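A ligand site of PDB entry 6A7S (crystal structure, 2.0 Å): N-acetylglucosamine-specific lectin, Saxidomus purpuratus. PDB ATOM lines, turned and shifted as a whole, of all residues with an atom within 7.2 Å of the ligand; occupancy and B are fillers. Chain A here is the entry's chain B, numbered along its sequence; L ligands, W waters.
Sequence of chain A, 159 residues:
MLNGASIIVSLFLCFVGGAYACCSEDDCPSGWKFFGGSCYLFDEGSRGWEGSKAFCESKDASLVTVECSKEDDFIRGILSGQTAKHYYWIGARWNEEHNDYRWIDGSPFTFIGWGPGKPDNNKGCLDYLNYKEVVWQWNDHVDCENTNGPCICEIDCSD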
ATOM      1  N   HIS A  86      23.897   5.180   6.562  1.00  0.00           N
ATOM      2  CA  HIS A  86      24.434   6.320   5.883  1.00  0.00           C
ATOM      3  C   HIS A  86      24.602   6.066   4.367  1.00  0.00           C
ATOM      4  O   HIS A  86      25.111   6.904   3.666  1.00  0.00           O
ATOM      5  CB  HIS A  86      25.726   6.810   6.628  1.00  0.00           C
ATOM      6  CG  HIS A  86      26.999   6.020   6.423  1.00  0.00           C
ATOM      7  ND1 HIS A  86      27.258   4.844   7.090  1.00  0.00           N
ATOM      8  CD2 HIS A  86      28.105   6.262   5.660  1.00  0.00           C
ATOM      9  CE1 HIS A  86      28.464   4.377   6.731  1.00  0.00           C
ATOM     10  NE2 HIS A  86      29.009   5.232   5.836  1.00  0.00           N
ATOM     11  N   TYR A  87      24.121   4.945   3.848  1.00  0.00           N
ATOM     12  CA  TYR A  87      24.040   4.783   2.425  1.00  0.00           C
ATOM     13  C   TYR A  87      22.953   3.760   2.073  1.00  0.00           C
ATOM     14  O   TYR A  87      22.732   2.827   2.815  1.00  0.00           O
ATOM     15  CB  TYR A  87      25.386   4.345   1.812  1.00  0.00           C
ATOM     16  CG  TYR A  87      26.006   3.110   2.396  1.00  0.00           C
ATOM     17  CD1 TYR A  87      26.780   3.184   3.536  1.00  0.00           C
ATOM     18  CD2 TYR A  87      25.837   1.842   1.816  1.00  0.00           C
ATOM     19  CE1 TYR A  87      27.323   2.061   4.128  1.00  0.00           C
ATOM     20  CE2 TYR A  87      26.395   0.699   2.387  1.00  0.00           C
ATOM     21  CZ  TYR A  87      27.149   0.817   3.550  1.00  0.00           C
ATOM     22  OH  TYR A  87      27.721  -0.271   4.145  1.00  0.00           O
ATOM     23  N   TYR A  88      22.380   3.941   0.879  1.00  0.00           N
ATOM     24  CA  TYR A  88      21.342   3.049   0.271  1.00  0.00           C
ATOM     25  C   TYR A  88      21.652   2.841  -1.211  1.00  0.00           C
ATOM     26  O   TYR A  88      21.838   3.785  -1.974  1.00  0.00           O
ATOM     27  CB  TYR A  88      19.951   3.645   0.342  1.00  0.00           C
ATOM     28  CG  TYR A  88      19.353   3.681   1.722  1.00  0.00           C
ATOM     29  CD1 TYR A  88      19.854   4.533   2.695  1.00  0.00           C
ATOM     30  CD2 TYR A  88      18.267   2.877   2.040  1.00  0.00           C
ATOM     31  CE1 TYR A  88      19.299   4.556   3.966  1.00  0.00           C
ATOM     32  CE2 TYR A  88      17.682   2.901   3.312  1.00  0.00           C
ATOM     33  CZ  TYR A  88      18.215   3.736   4.277  1.00  0.00           C
ATOM     34  OH  TYR A  88      17.649   3.732   5.532  1.00  0.00           O
ATOM     35  N   TRP A  89      21.720   1.575  -1.618  1.00  0.00           N
ATOM     36  CA  TRP A  89      22.000   1.244  -3.023  1.00  0.00           C
ATOM     37  C   TRP A  89      20.849   1.670  -3.942  1.00  0.00           C
ATOM     38  O   TRP A  89      19.694   1.575  -3.557  1.00  0.00           O
ATOM     39  CB  TRP A  89      22.283  -0.248  -3.142  1.00  0.00           C
ATOM     40  CG  TRP A  89      23.492  -0.716  -2.407  1.00  0.00           C
ATOM     41  CD1 TRP A  89      23.532  -1.683  -1.446  1.00  0.00           C
ATOM     42  CD2 TRP A  89      24.840  -0.234  -2.561  1.00  0.00           C
ATOM     43  NE1 TRP A  89      24.814  -1.835  -0.997  1.00  0.00           N
ATOM     44  CE2 TRP A  89      25.625  -0.964  -1.653  1.00  0.00           C
ATOM     45  CE3 TRP A  89      25.443   0.722  -3.362  1.00  0.00           C
ATOM     46  CZ2 TRP A  89      26.982  -0.704  -1.474  1.00  0.00           C
ATOM     47  CZ3 TRP A  89      26.804   0.928  -3.233  1.00  0.00           C
ATOM     48  CH2 TRP A  89      27.555   0.187  -2.325  1.00  0.00           C
ATOM     49  N   LYS A 118      31.709  14.446  -6.584  1.00  0.00           N
ATOM     50  CA  LYS A 118      31.436  13.120  -7.200  1.00  0.00           C
ATOM     51  C   LYS A 118      31.118  13.296  -8.672  1.00  0.00           C
ATOM     52  O   LYS A 118      30.648  14.362  -9.058  1.00  0.00           O
ATOM     53  CB  LYS A 118      30.276  12.452  -6.449  1.00  0.00           C
ATOM     54  CG  LYS A 118      30.462  12.361  -4.942  1.00  0.00           C
ATOM     55  CD  LYS A 118      31.769  11.721  -4.552  1.00  0.00           C
ATOM     56  CE  LYS A 118      32.011  11.560  -3.070  1.00  0.00           C
ATOM     57  NZ  LYS A 118      33.077  10.571  -2.800  1.00  0.00           N
ATOM     58  N   ASP A 120      33.846   9.893  -8.276  1.00  0.00           N
ATOM     59  CA  ASP A 120      35.270   9.592  -8.138  1.00  0.00           C
ATOM     60  C   ASP A 120      35.766   8.906  -9.426  1.00  0.00           C
ATOM     61  O   ASP A 120      36.924   8.891  -9.694  1.00  0.00           O
ATOM     62  CB  ASP A 120      35.507   8.707  -6.910  1.00  0.00           C
ATOM     63  CG  ASP A 120      35.090   9.412  -5.612  1.00  0.00           C
ATOM     64  OD1 ASP A 120      35.747  10.397  -5.280  1.00  0.00           O
ATOM     65  OD2 ASP A 120      34.018   9.049  -5.033  1.00  0.00           O
ATOM     66  N   ASN A 122      35.436   5.394 -10.232  1.00  0.00           N
ATOM     67  CA  ASN A 122      36.088   4.192  -9.794  1.00  0.00           C
ATOM     68  C   ASN A 122      35.406   2.984 -10.444  1.00  0.00           C
ATOM     69  O   ASN A 122      35.542   1.865 -10.015  1.00  0.00           O
ATOM     70  CB  ASN A 122      36.109   4.136  -8.253  1.00  0.00           C
ATOM     71  CG  ASN A 122      34.746   4.269  -7.611  1.00  0.00           C
ATOM     72  OD1 ASN A 122      33.734   3.997  -8.274  1.00  0.00           O
ATOM     73  ND2 ASN A 122      34.710   4.658  -6.331  1.00  0.00           N
ATOM     74  N   CYS A 125      29.515   1.286  -8.260  1.00  0.00           N
ATOM     75  CA  CYS A 125      28.043   1.189  -8.162  1.00  0.00           C
ATOM     76  C   CYS A 125      27.513   2.340  -7.314  1.00  0.00           C
ATOM     77  O   CYS A 125      28.176   2.773  -6.364  1.00  0.00           O
ATOM     78  CB  CYS A 125      27.656  -0.130  -7.503  1.00  0.00           C
ATOM     79  SG  CYS A 125      27.857  -1.552  -8.614  1.00  0.00           S
ATOM     80  N   LEU A 126      26.324   2.835  -7.610  1.00  0.00           N
ATOM     81  CA  LEU A 126      25.887   4.081  -7.022  1.00  0.00           C
ATOM     82  C   LEU A 126      25.057   3.788  -5.774  1.00  0.00           C
ATOM     83  O   LEU A 126      24.291   2.788  -5.703  1.00  0.00           O
ATOM     84  CB  LEU A 126      25.109   4.926  -8.026  1.00  0.00           C
ATOM     85  CG  LEU A 126      25.951   5.838  -8.915  1.00  0.00           C
ATOM     86  CD1 LEU A 126      26.583   5.053 -10.064  1.00  0.00           C
ATOM     87  CD2 LEU A 126      25.083   6.950  -9.441  1.00  0.00           C
ATOM     88  N   ASP A 127      25.224   4.698  -4.817  1.00  0.00           N
ATOM     89  CA  ASP A 127      24.367   4.797  -3.649  1.00  0.00           C
ATOM     90  C   ASP A 127      23.950   6.242  -3.432  1.00  0.00           C
ATOM     91  O   ASP A 127      24.455   7.119  -4.065  1.00  0.00           O
ATOM     92  CB  ASP A 127      25.021   4.177  -2.422  1.00  0.00           C
ATOM     93  CG  ASP A 127      26.417   4.714  -2.066  1.00  0.00           C
ATOM     94  OD1 ASP A 127      26.682   5.858  -2.440  1.00  0.00           O
ATOM     95  OD2 ASP A 127      27.140   4.003  -1.315  1.00  0.00           O
ATOM     96  N   TYR A 128      22.890   6.438  -2.656  1.00  0.00           N
ATOM     97  CA  TYR A 128      22.713   7.665  -1.965  1.00  0.00           C
ATOM     98  C   TYR A 128      23.609   7.599  -0.744  1.00  0.00           C
ATOM     99  O   TYR A 128      23.614   6.589  -0.079  1.00  0.00           O
ATOM    100  CB  TYR A 128      21.252   7.893  -1.535  1.00  0.00           C
ATOM    101  CG  TYR A 128      20.451   8.567  -2.607  1.00  0.00           C
ATOM    102  CD1 TYR A 128      19.837   7.831  -3.605  1.00  0.00           C
ATOM    103  CD2 TYR A 128      20.334   9.940  -2.662  1.00  0.00           C
ATOM    104  CE1 TYR A 128      19.128   8.432  -4.629  1.00  0.00           C
ATOM    105  CE2 TYR A 128      19.610  10.561  -3.664  1.00  0.00           C
ATOM    106  CZ  TYR A 128      19.022   9.803  -4.673  1.00  0.00           C
ATOM    107  OH  TYR A 128      18.343  10.402  -5.697  1.00  0.00           O
ATOM    108  N   LEU A 129      24.400   8.638  -0.499  1.00  0.00           N
ATOM    109  CA  LEU A 129      25.360   8.611   0.588  1.00  0.00           C
ATOM    110  C   LEU A 129      25.117   9.823   1.473  1.00  0.00           C
ATOM    111  O   LEU A 129      24.821  10.901   1.008  1.00  0.00           O
ATOM    112  CB  LEU A 129      26.779   8.640   0.020  1.00  0.00           C
ATOM    113  CG  LEU A 129      27.956   8.789   0.993  1.00  0.00           C
ATOM    114  CD1 LEU A 129      28.069   7.586   1.922  1.00  0.00           C
ATOM    115  CD2 LEU A 129      29.276   8.921   0.208  1.00  0.00           C
ATOM    116  N   ASN A 130      25.291   9.631   2.778  1.00  0.00           N
ATOM    117  CA  ASN A 130      25.236  10.696   3.737  1.00  0.00           C
ATOM    118  C   ASN A 130      26.579  10.683   4.464  1.00  0.00           C
ATOM    119  O   ASN A 130      26.734   9.917   5.390  1.00  0.00           O
ATOM    120  CB  ASN A 130      24.103  10.561   4.734  1.00  0.00           C
ATOM    121  CG  ASN A 130      23.995  11.791   5.611  1.00  0.00           C
ATOM    122  OD1 ASN A 130      24.282  12.905   5.155  1.00  0.00           O
ATOM    123  ND2 ASN A 130      23.534  11.592   6.824  1.00  0.00           N
ATOM    124  N   TYR A 131      27.554  11.461   3.984  1.00  0.00           N
ATOM    125  CA  TYR A 131      28.880  11.437   4.602  1.00  0.00           C
ATOM    126  C   TYR A 131      29.598  12.739   4.291  1.00  0.00           C
ATOM    127  O   TYR A 131      29.823  13.032   3.128  1.00  0.00           O
ATOM    128  CB  TYR A 131      29.738  10.277   4.056  1.00  0.00           C
ATOM    129  CG  TYR A 131      31.089  10.120   4.721  1.00  0.00           C
ATOM    130  CD1 TYR A 131      31.190   9.943   6.093  1.00  0.00           C
ATOM    131  CD2 TYR A 131      32.278  10.188   3.987  1.00  0.00           C
ATOM    132  CE1 TYR A 131      32.412   9.803   6.719  1.00  0.00           C
ATOM    133  CE2 TYR A 131      33.514  10.073   4.606  1.00  0.00           C
ATOM    134  CZ  TYR A 131      33.577   9.864   5.966  1.00  0.00           C
ATOM    135  OH  TYR A 131      34.774   9.761   6.587  1.00  0.00           O
ATOM    136  N   LYS A 132      30.014  13.469   5.332  1.00  0.00           N
ATOM    137  CA  LYS A 132      30.721  14.746   5.210  1.00  0.00           C
ATOM    138  C   LYS A 132      29.871  15.695   4.361  1.00  0.00           C
ATOM    139  O   LYS A 132      28.723  15.952   4.680  1.00  0.00           O
ATOM    140  CB  LYS A 132      32.137  14.598   4.634  1.00  0.00           C
ATOM    141  CG  LYS A 132      33.021  13.488   5.174  1.00  0.00           C
ATOM    142  CD  LYS A 132      33.876  13.900   6.304  1.00  0.00           C
ATOM    143  CE  LYS A 132      33.011  14.261   7.487  1.00  0.00           C
ATOM    144  NZ  LYS A 132      33.804  14.308   8.734  1.00  0.00           N
ATOM    145  N   VAL A 134      28.725  15.153   1.415  1.00  0.00           N
ATOM    146  CA  VAL A 134      27.721  14.485   0.594  1.00  0.00           C
ATOM    147  C   VAL A 134      26.483  14.278   1.448  1.00  0.00           C
ATOM    148  O   VAL A 134      26.496  13.474   2.393  1.00  0.00           O
ATOM    149  CB  VAL A 134      28.240  13.169   0.005  1.00  0.00           C
ATOM    150  CG1 VAL A 134      27.187  12.465  -0.850  1.00  0.00           C
ATOM    151  CG2 VAL A 134      29.491  13.440  -0.813  1.00  0.00           C
ATOM    152  N   ASN A 139      26.917   8.802  -4.722  1.00  0.00           N
ATOM    153  CA  ASN A 139      28.326   8.461  -4.725  1.00  0.00           C
ATOM    154  C   ASN A 139      28.501   7.182  -5.541  1.00  0.00           C
ATOM    155  O   ASN A 139      27.577   6.340  -5.562  1.00  0.00           O
ATOM    156  CB  ASN A 139      28.925   8.294  -3.317  1.00  0.00           C
ATOM    157  CG  ASN A 139      30.385   7.841  -3.352  1.00  0.00           C
ATOM    158  OD1 ASN A 139      31.240   8.433  -4.014  1.00  0.00           O
ATOM    159  ND2 ASN A 139      30.645   6.738  -2.664  1.00  0.00           N
ATOM    160  N   ASP A 140      29.688   7.059  -6.167  1.00  0.00           N
ATOM    161  CA  ASP A 140      30.102   5.819  -6.750  1.00  0.00           C
ATOM    162  C   ASP A 140      31.004   5.099  -5.752  1.00  0.00           C
ATOM    163  O   ASP A 140      32.048   5.619  -5.323  1.00  0.00           O
ATOM    164  CB  ASP A 140      30.788   5.978  -8.120  1.00  0.00           C
ATOM    165  CG  ASP A 140      31.894   7.014  -8.224  1.00  0.00           C
ATOM    166  OD1 ASP A 140      32.079   7.837  -7.281  1.00  0.00           O
ATOM    167  OD2 ASP A 140      32.603   6.961  -9.290  1.00  0.00           O
ATOM    168  N   HIS A 141      30.571   3.874  -5.397  1.00  0.00           N
ATOM    169  CA  HIS A 141      31.312   3.017  -4.493  1.00  0.00           C
ATOM    170  C   HIS A 141      32.029   1.935  -5.273  1.00  0.00           C
ATOM    171  O   HIS A 141      31.412   1.216  -6.058  1.00  0.00           O
ATOM    172  CB  HIS A 141      30.405   2.363  -3.460  1.00  0.00           C
ATOM    173  CG  HIS A 141      31.160   1.703  -2.378  1.00  0.00           C
ATOM    174  ND1 HIS A 141      31.847   2.431  -1.395  1.00  0.00           N
ATOM    175  CD2 HIS A 141      31.359   0.387  -2.113  1.00  0.00           C
ATOM    176  CE1 HIS A 141      32.428   1.579  -0.595  1.00  0.00           C
ATOM    177  NE2 HIS A 141      32.095   0.317  -0.967  1.00  0.00           N
ATOM    178  N   VAL A 142      33.313   1.760  -4.926  1.00  0.00           N
ATOM    179  CA  VAL A 142      34.205   0.920  -5.726  1.00  0.00           C
ATOM    180  C   VAL A 142      33.817  -0.573  -5.682  1.00  0.00           C
ATOM    181  O   VAL A 142      34.136  -1.283  -6.626  1.00  0.00           O
ATOM    182  CB  VAL A 142      35.668   1.119  -5.282  1.00  0.00           C
ATOM    183  CG1 VAL A 142      35.899   0.652  -3.861  1.00  0.00           C
ATOM    184  CG2 VAL A 142      36.645   0.474  -6.253  1.00  0.00           C
ATOM    185  N   ASP A 143      33.179  -1.014  -4.589  1.00  0.00           N
ATOM    186  CA  ASP A 143      32.846  -2.411  -4.274  1.00  0.00           C
ATOM    187  C   ASP A 143      31.353  -2.666  -4.510  1.00  0.00           C
ATOM    188  O   ASP A 143      30.531  -2.336  -3.666  1.00  0.00           O
ATOM    189  CB  ASP A 143      33.189  -2.735  -2.820  1.00  0.00           C
ATOM    190  CG  ASP A 143      32.795  -4.120  -2.369  1.00  0.00           C
ATOM    191  OD1 ASP A 143      32.629  -5.022  -3.272  1.00  0.00           O
ATOM    192  OD2 ASP A 143      32.643  -4.302  -1.143  1.00  0.00           O
ATOM    193  N   THR A 147      30.083  -4.792  -0.059  1.00  0.00           N
ATOM    194  CA  THR A 147      29.737  -3.748   0.849  1.00  0.00           C
ATOM    195  C   THR A 147      28.239  -3.806   1.147  1.00  0.00           C
ATOM    196  O   THR A 147      27.432  -3.513   0.315  1.00  0.00           O
ATOM    197  CB  THR A 147      30.203  -2.378   0.371  1.00  0.00           C
ATOM    198  OG1 THR A 147      31.631  -2.409   0.187  1.00  0.00           O
ATOM    199  CG2 THR A 147      29.788  -1.306   1.347  1.00  0.00           C
HETATM  200  C1  LIG L   1      32.484   6.340   1.927  1.00  0.00           C
HETATM  201  C2  LIG L   1      31.789   5.856   0.645  1.00  0.00           C
HETATM  202  C3  LIG L   1      33.038   5.462  -0.124  1.00  0.00           C
HETATM  203  C4  LIG L   1      34.021   6.678  -0.142  1.00  0.00           C
HETATM  204  C5  LIG L   1      34.166   7.418   1.175  1.00  0.00           C
HETATM  205  C6  LIG L   1      35.129   8.633   1.248  1.00  0.00           C
HETATM  206  C7  LIG L   1      29.896   4.347   0.251  1.00  0.00           C
HETATM  207  C8  LIG L   1      29.406   2.954   0.602  1.00  0.00           C
HETATM  208  N1  LIG L   1      31.033   4.647   0.868  1.00  0.00           N
HETATM  209  O1  LIG L   1      32.181   5.917   3.222  1.00  0.00           O
HETATM  210  O2  LIG L   1      32.682   4.949  -1.406  1.00  0.00           O
HETATM  211  O3  LIG L   1      33.457   7.464  -1.183  1.00  0.00           O
HETATM  212  O4  LIG L   1      32.842   7.708   1.711  1.00  0.00           O
HETATM  213  O5  LIG L   1      36.449   8.183   0.892  1.00  0.00           O
HETATM  214  O6  LIG L   1      29.380   5.068  -0.562  1.00  0.00           O
HETATM  215  O   HOH W   1      37.310   7.522   3.314  1.00  0.00           O
HETATM  216  O   HOH W   2      34.416   6.755  -3.714  1.00  0.00           O
HETATM  217  O   HOH W   3      32.310  10.203  -0.008  1.00  0.00           O
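A ring nitrogen (ND1) of His 141 is in hydrogen-bond range of an oxygen (O2) of the ligand (2.7 Å). ND2 of Asn 139 lies within hydrogen-bond range of O6 of the ligand (3.0 Å). An oxygen (O6) of the ligand sits close to the side-chain carboxylate (OD2) of Asp 127 (2.6 Å).
The backbone NH (N) of His 141 lies within hydrogen-bond range of the backbone carbonyl oxygen (O) of Cys 125. A ring nitrogen (NE2) of His 141 lies within hydrogen-bond range of the side-chain hydroxyl of Thr 147 (3.0 Å). OD2 of Asp 120 lies within salt-bridge range of NZ of Lys 118, 2.9 Å away. The side-chain amino group (NZ) of Lys 118 lies within hydrogen-bond range of the side-chain amide oxygen (OD1) of Asn 139, at 3.1 Å. The side-chain amide oxygen of Asn 139 lies close to the side-chain carboxylate of Asp 140 (3.4 Å). N of Asp 127 is in hydrogen-bond range of O of Asn 139 (3.0 Å). The side-chain amide oxygen of Asn 139 sits close to the side-chain carboxylate of Asp 120 (3.0 Å).
Merely in contact with the ligand: Tyr 87 (3.8 Å), Lys 118 (3.5 Å), Leu 129 (3.8 Å) and Tyr 131 (3.4 Å). Hydrophobic or aromatic side chains within 4 Å of the ligand: Tyr 87, Leu 129, Tyr 131 and His 141. Seven residues have an atom within 4 Å of the ligand: Tyr 87, Lys 118, Asp 127, Leu 129, Tyr 131, Asn 139 and His 141.
Water W2 lies within hydrogen-bond range of the side-chain carboxylate of Asp 120 (2.7 Å), an oxygen (O3) of the ligand (2.8 Å), the backbone carbonyl oxygen of Asp 140 (3.1 Å) and the side-chain amide nitrogen of Asn 122 (3.4 Å). Water W3 lies within hydrogen-bond range of NZ of Lys 118 (2.9 Å) and O4 of the ligand (3.1 Å).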
